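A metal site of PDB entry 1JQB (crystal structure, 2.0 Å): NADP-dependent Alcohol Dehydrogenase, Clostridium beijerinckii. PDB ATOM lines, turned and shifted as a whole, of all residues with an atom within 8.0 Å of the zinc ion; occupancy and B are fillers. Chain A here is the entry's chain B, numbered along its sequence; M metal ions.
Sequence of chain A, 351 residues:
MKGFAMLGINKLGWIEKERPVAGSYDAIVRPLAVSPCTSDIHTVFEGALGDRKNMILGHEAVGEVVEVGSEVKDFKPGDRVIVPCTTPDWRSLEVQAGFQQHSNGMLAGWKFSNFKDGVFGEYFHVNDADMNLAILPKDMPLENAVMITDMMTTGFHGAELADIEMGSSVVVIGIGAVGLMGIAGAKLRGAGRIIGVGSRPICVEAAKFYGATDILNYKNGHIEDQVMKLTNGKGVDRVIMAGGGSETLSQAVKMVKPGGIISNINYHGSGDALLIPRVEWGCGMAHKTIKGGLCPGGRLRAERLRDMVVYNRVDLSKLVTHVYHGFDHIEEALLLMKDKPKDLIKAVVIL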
ATOM      1  N   SER A  35     -29.316  34.861 -22.800  1.00  0.00           N
ATOM      2  CA  SER A  35     -28.450  35.334 -21.719  1.00  0.00           C
ATOM      3  C   SER A  35     -27.007  34.926 -21.918  1.00  0.00           C
ATOM      4  O   SER A  35     -26.712  33.764 -22.208  1.00  0.00           O
ATOM      5  CB  SER A  35     -28.957  34.812 -20.372  1.00  0.00           C
ATOM      6  OG  SER A  35     -28.107  35.239 -19.301  1.00  0.00           O
ATOM      7  N   PRO A  36     -26.077  35.888 -21.791  1.00  0.00           N
ATOM      8  CA  PRO A  36     -24.647  35.594 -21.965  1.00  0.00           C
ATOM      9  C   PRO A  36     -24.158  34.804 -20.751  1.00  0.00           C
ATOM     10  O   PRO A  36     -24.617  35.024 -19.625  1.00  0.00           O
ATOM     11  CB  PRO A  36     -24.032  36.984 -22.049  1.00  0.00           C
ATOM     12  CG  PRO A  36     -24.876  37.758 -21.089  1.00  0.00           C
ATOM     13  CD  PRO A  36     -26.283  37.311 -21.465  1.00  0.00           C
ATOM     14  N   CYS A  37     -23.215  33.894 -20.973  1.00  0.00           N
ATOM     15  CA  CYS A  37     -22.681  33.069 -19.897  1.00  0.00           C
ATOM     16  C   CYS A  37     -21.194  33.292 -19.708  1.00  0.00           C
ATOM     17  O   CYS A  37     -20.477  33.669 -20.645  1.00  0.00           O
ATOM     18  CB  CYS A  37     -22.931  31.590 -20.193  1.00  0.00           C
ATOM     19  SG  CYS A  37     -22.340  30.451 -18.889  1.00  0.00           S
ATOM     20  N   THR A  38     -20.721  33.046 -18.483  1.00  0.00           N
ATOM     21  CA  THR A  38     -19.309  33.218 -18.184  1.00  0.00           C
ATOM     22  C   THR A  38     -18.501  32.303 -19.087  1.00  0.00           C
ATOM     23  O   THR A  38     -17.329  32.557 -19.356  1.00  0.00           O
ATOM     24  CB  THR A  38     -19.017  32.886 -16.697  1.00  0.00           C
ATOM     25  OG1 THR A  38     -19.303  31.506 -16.442  1.00  0.00           O
ATOM     26  CG2 THR A  38     -19.877  33.759 -15.784  1.00  0.00           C
ATOM     27  N   SER A  39     -19.135  31.229 -19.563  1.00  0.00           N
ATOM     28  CA  SER A  39     -18.462  30.293 -20.458  1.00  0.00           C
ATOM     29  C   SER A  39     -18.305  30.885 -21.863  1.00  0.00           C
ATOM     30  O   SER A  39     -17.429  30.485 -22.623  1.00  0.00           O
ATOM     31  CB  SER A  39     -19.240  28.977 -20.527  1.00  0.00           C
ATOM     32  OG  SER A  39     -20.491  29.158 -21.154  1.00  0.00           O
ATOM     33  N   ASP A  40     -19.167  31.850 -22.210  1.00  0.00           N
ATOM     34  CA  ASP A  40     -19.078  32.497 -23.517  1.00  0.00           C
ATOM     35  C   ASP A  40     -17.798  33.342 -23.486  1.00  0.00           C
ATOM     36  O   ASP A  40     -16.997  33.324 -24.418  1.00  0.00           O
ATOM     37  CB  ASP A  40     -20.271  33.436 -23.765  1.00  0.00           C
ATOM     38  CG  ASP A  40     -21.568  32.676 -24.049  1.00  0.00           C
ATOM     39  OD1 ASP A  40     -21.598  31.871 -25.007  1.00  0.00           O
ATOM     40  OD2 ASP A  40     -22.559  32.922 -23.330  1.00  0.00           O
ATOM     41  N   GLY A  58     -23.496  31.742 -27.370  1.00  0.00           N
ATOM     42  CA  GLY A  58     -24.706  31.623 -26.588  1.00  0.00           C
ATOM     43  C   GLY A  58     -25.286  30.229 -26.523  1.00  0.00           C
ATOM     44  O   GLY A  58     -25.214  29.473 -27.488  1.00  0.00           O
ATOM     45  N   HIS A  59     -25.860  29.876 -25.370  1.00  0.00           N
ATOM     46  CA  HIS A  59     -26.470  28.562 -25.195  1.00  0.00           C
ATOM     47  C   HIS A  59     -27.551  28.624 -24.142  1.00  0.00           C
ATOM     48  O   HIS A  59     -27.943  27.602 -23.579  1.00  0.00           O
ATOM     49  CB  HIS A  59     -25.436  27.505 -24.815  1.00  0.00           C
ATOM     50  CG  HIS A  59     -24.659  27.840 -23.587  1.00  0.00           C
ATOM     51  ND1 HIS A  59     -23.357  28.293 -23.634  1.00  0.00           N
ATOM     52  CD2 HIS A  59     -25.004  27.820 -22.272  1.00  0.00           C
ATOM     53  CE1 HIS A  59     -22.935  28.525 -22.400  1.00  0.00           C
ATOM     54  NE2 HIS A  59     -23.914  28.248 -21.557  1.00  0.00           N
ATOM     55  N   GLU A  60     -28.020  29.830 -23.868  1.00  0.00           N
ATOM     56  CA  GLU A  60     -29.063  30.052 -22.883  1.00  0.00           C
ATOM     57  C   GLU A  60     -30.165  30.874 -23.523  1.00  0.00           C
ATOM     58  O   GLU A  60     -29.983  32.074 -23.774  1.00  0.00           O
ATOM     59  CB  GLU A  60     -28.493  30.800 -21.673  1.00  0.00           C
ATOM     60  CG  GLU A  60     -27.521  29.966 -20.871  1.00  0.00           C
ATOM     61  CD  GLU A  60     -26.915  30.744 -19.732  1.00  0.00           C
ATOM     62  OE1 GLU A  60     -27.681  31.315 -18.919  1.00  0.00           O
ATOM     63  OE2 GLU A  60     -25.672  30.798 -19.645  1.00  0.00           O
ATOM     64  N   CYS A  85     -29.639  24.048 -22.128  1.00  0.00           N
ATOM     65  CA  CYS A  85     -28.364  24.267 -22.818  1.00  0.00           C
ATOM     66  C   CYS A  85     -27.718  22.970 -23.289  1.00  0.00           C
ATOM     67  O   CYS A  85     -26.933  22.962 -24.242  1.00  0.00           O
ATOM     68  CB  CYS A  85     -27.381  25.035 -21.916  1.00  0.00           C
ATOM     69  SG  CYS A  85     -26.858  24.143 -20.435  1.00  0.00           S
ATOM     70  N   TRP A 110     -23.403  18.942 -24.708  1.00  0.00           N
ATOM     71  CA  TRP A 110     -23.430  20.398 -24.752  1.00  0.00           C
ATOM     72  C   TRP A 110     -22.958  20.803 -26.136  1.00  0.00           C
ATOM     73  O   TRP A 110     -21.762  20.763 -26.428  1.00  0.00           O
ATOM     74  CB  TRP A 110     -22.508  20.952 -23.666  1.00  0.00           C
ATOM     75  CG  TRP A 110     -22.294  22.428 -23.735  1.00  0.00           C
ATOM     76  CD1 TRP A 110     -23.259  23.387 -23.863  1.00  0.00           C
ATOM     77  CD2 TRP A 110     -21.034  23.112 -23.706  1.00  0.00           C
ATOM     78  NE1 TRP A 110     -22.673  24.631 -23.917  1.00  0.00           N
ATOM     79  CE2 TRP A 110     -21.317  24.487 -23.820  1.00  0.00           C
ATOM     80  CE3 TRP A 110     -19.709  22.691 -23.583  1.00  0.00           C
ATOM     81  CZ2 TRP A 110     -20.303  25.457 -23.830  1.00  0.00           C
ATOM     82  CZ3 TRP A 110     -18.704  23.661 -23.594  1.00  0.00           C
ATOM     83  CH2 TRP A 110     -19.007  25.020 -23.711  1.00  0.00           C
ATOM     84  N   SER A 113     -22.658  26.578 -29.159  1.00  0.00           N
ATOM     85  CA  SER A 113     -21.414  27.320 -28.996  1.00  0.00           C
ATOM     86  C   SER A 113     -20.276  26.456 -28.451  1.00  0.00           C
ATOM     87  O   SER A 113     -19.533  26.877 -27.576  1.00  0.00           O
ATOM     88  CB  SER A 113     -21.621  28.517 -28.051  1.00  0.00           C
ATOM     89  OG  SER A 113     -21.552  28.121 -26.689  1.00  0.00           O
ATOM     90  N   VAL A 146     -35.267  31.866 -18.872  1.00  0.00           N
ATOM     91  CA  VAL A 146     -33.923  31.699 -19.405  1.00  0.00           C
ATOM     92  C   VAL A 146     -32.961  31.165 -18.340  1.00  0.00           C
ATOM     93  O   VAL A 146     -32.010  30.456 -18.646  1.00  0.00           O
ATOM     94  CB  VAL A 146     -33.349  33.023 -19.948  1.00  0.00           C
ATOM     95  CG1 VAL A 146     -31.949  32.798 -20.485  1.00  0.00           C
ATOM     96  CG2 VAL A 146     -34.252  33.593 -21.050  1.00  0.00           C
ATOM     97  N   THR A 149     -32.452  27.227 -18.343  1.00  0.00           N
ATOM     98  CA  THR A 149     -31.607  26.583 -19.337  1.00  0.00           C
ATOM     99  C   THR A 149     -30.198  26.201 -18.888  1.00  0.00           C
ATOM    100  O   THR A 149     -29.631  25.253 -19.421  1.00  0.00           O
ATOM    101  CB  THR A 149     -31.514  27.451 -20.591  1.00  0.00           C
ATOM    102  OG1 THR A 149     -30.763  28.635 -20.287  1.00  0.00           O
ATOM    103  CG2 THR A 149     -32.924  27.861 -21.045  1.00  0.00           C
ATOM    104  N   ASP A 150     -29.615  26.939 -17.940  1.00  0.00           N
ATOM    105  CA  ASP A 150     -28.284  26.589 -17.473  1.00  0.00           C
ATOM    106  C   ASP A 150     -28.024  26.867 -16.007  1.00  0.00           C
ATOM    107  O   ASP A 150     -27.543  25.987 -15.297  1.00  0.00           O
ATOM    108  CB  ASP A 150     -27.193  27.298 -18.294  1.00  0.00           C
ATOM    109  CG  ASP A 150     -25.806  26.811 -17.897  1.00  0.00           C
ATOM    110  OD1 ASP A 150     -24.815  27.510 -18.169  1.00  0.00           O
ATOM    111  OD2 ASP A 150     -25.696  25.722 -17.305  1.00  0.00           O
ATOM    112  N   MET A 151     -28.325  28.067 -15.533  1.00  0.00           N
ATOM    113  CA  MET A 151     -28.062  28.375 -14.132  1.00  0.00           C
ATOM    114  C   MET A 151     -28.763  27.421 -13.155  1.00  0.00           C
ATOM    115  O   MET A 151     -28.132  26.871 -12.251  1.00  0.00           O
ATOM    116  CB  MET A 151     -28.471  29.827 -13.826  1.00  0.00           C
ATOM    117  CG  MET A 151     -27.714  30.889 -14.632  1.00  0.00           C
ATOM    118  SD  MET A 151     -25.904  30.827 -14.475  1.00  0.00           S
ATOM    119  CE  MET A 151     -25.420  30.042 -15.992  1.00  0.00           C
ATOM    120  N   THR A 154     -27.624  23.593 -13.706  1.00  0.00           N
ATOM    121  CA  THR A 154     -26.237  23.385 -13.291  1.00  0.00           C
ATOM    122  C   THR A 154     -26.113  23.464 -11.767  1.00  0.00           C
ATOM    123  O   THR A 154     -25.541  22.582 -11.137  1.00  0.00           O
ATOM    124  CB  THR A 154     -25.321  24.430 -13.942  1.00  0.00           C
ATOM    125  OG1 THR A 154     -25.360  24.257 -15.367  1.00  0.00           O
ATOM    126  CG2 THR A 154     -23.867  24.262 -13.474  1.00  0.00           C
ATOM    127  N   VAL A 178     -24.368  30.476 -10.782  1.00  0.00           N
ATOM    128  CA  VAL A 178     -24.336  29.027 -10.634  1.00  0.00           C
ATOM    129  C   VAL A 178     -24.286  28.634  -9.151  1.00  0.00           C
ATOM    130  O   VAL A 178     -25.016  27.742  -8.714  1.00  0.00           O
ATOM    131  CB  VAL A 178     -23.127  28.435 -11.397  1.00  0.00           C
ATOM    132  CG1 VAL A 178     -22.967  26.942 -11.081  1.00  0.00           C
ATOM    133  CG2 VAL A 178     -23.346  28.634 -12.898  1.00  0.00           C
ATOM    134  N   CYS A 295     -24.081  19.919 -16.544  1.00  0.00           N
ATOM    135  CA  CYS A 295     -25.500  19.865 -16.199  1.00  0.00           C
ATOM    136  C   CYS A 295     -26.309  18.987 -17.153  1.00  0.00           C
ATOM    137  O   CYS A 295     -25.988  18.896 -18.340  1.00  0.00           O
ATOM    138  CB  CYS A 295     -26.102  21.266 -16.236  1.00  0.00           C
ATOM    139  SG  CYS A 295     -26.028  22.000 -17.892  1.00  0.00           S
ATOM    140  N   MET A 337     -20.536  40.931 -19.334  1.00  0.00           N
ATOM    141  CA  MET A 337     -20.177  39.725 -18.588  1.00  0.00           C
ATOM    142  C   MET A 337     -18.674  39.636 -18.436  1.00  0.00           C
ATOM    143  O   MET A 337     -18.168  38.876 -17.603  1.00  0.00           O
ATOM    144  CB  MET A 337     -20.695  38.469 -19.288  1.00  0.00           C
ATOM    145  CG  MET A 337     -22.174  38.147 -19.052  1.00  0.00           C
ATOM    146  SD  MET A 337     -22.609  37.904 -17.306  1.00  0.00           S
ATOM    147  CE  MET A 337     -22.224  36.162 -17.091  1.00  0.00           C
ATOM    148  N   LYS A 346     -26.754  38.150 -13.488  1.00  0.00           N
ATOM    149  CA  LYS A 346     -27.039  37.630 -14.829  1.00  0.00           C
ATOM    150  C   LYS A 346     -27.773  38.694 -15.648  1.00  0.00           C
ATOM    151  O   LYS A 346     -28.594  39.437 -15.122  1.00  0.00           O
ATOM    152  CB  LYS A 346     -27.916  36.377 -14.764  1.00  0.00           C
ATOM    153  CG  LYS A 346     -27.199  35.110 -14.295  1.00  0.00           C
ATOM    154  CD  LYS A 346     -26.216  34.588 -15.337  1.00  0.00           C
ATOM    155  CE  LYS A 346     -26.928  34.111 -16.587  1.00  0.00           C
ATOM    156  NZ  LYS A 346     -25.999  33.420 -17.535  1.00  0.00           N
HETATM  157 ZN    ZN M   1     -24.266  28.982 -19.461  1.00  0.00          ZN
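The zinc ion is bound by the side-chain carboxylate of Asp 150 (2.0 Å), a ring nitrogen (NE2) of His 59 (2.2 Å), the side-chain carboxylate of Glu 60 (2.3 Å) and the side-chain sulfur of Cys 37 (2.5 Å).
The zinc ion has four donor atoms within binding distance.
CE of Met 151 touches the zinc ion, at 3.8 Å.
Within 4 Å of the zinc ion: Cys 37, His 59, Glu 60, Asp 150 and Met 151.
The nearest printed residue that does not touch the zinc ion is Ser 39 (4.1 Å).
The side-chain hydroxyl (OG1) of Thr 154 sits at hydrogen-bond distance from the side-chain carboxylate (OD2) of Asp 150 (2.5 Å).
OD2 of Asp 150 is in hydrogen-bond range of SG of Cys 295 (3.8 Å).
OG of Ser 39 sits close to SG of Cys 37, 3.2 Å away.
The side-chain carboxylate (OD2) of Asp 150 is in hydrogen-bond range of the side-chain sulfur (SG) of Cys 85, 3.7 Å away.
NZ of Lys 346 is in salt-bridge range of OE1 of Glu 60, 3.0 Å away.
The backbone NH (N) of Cys 37 sits at hydrogen-bond distance from the side-chain carboxylate (OD2) of Asp 40 (2.6 Å).
N of Ser 35 sits at hydrogen-bond distance from O of Glu 60, at 3.0 Å.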
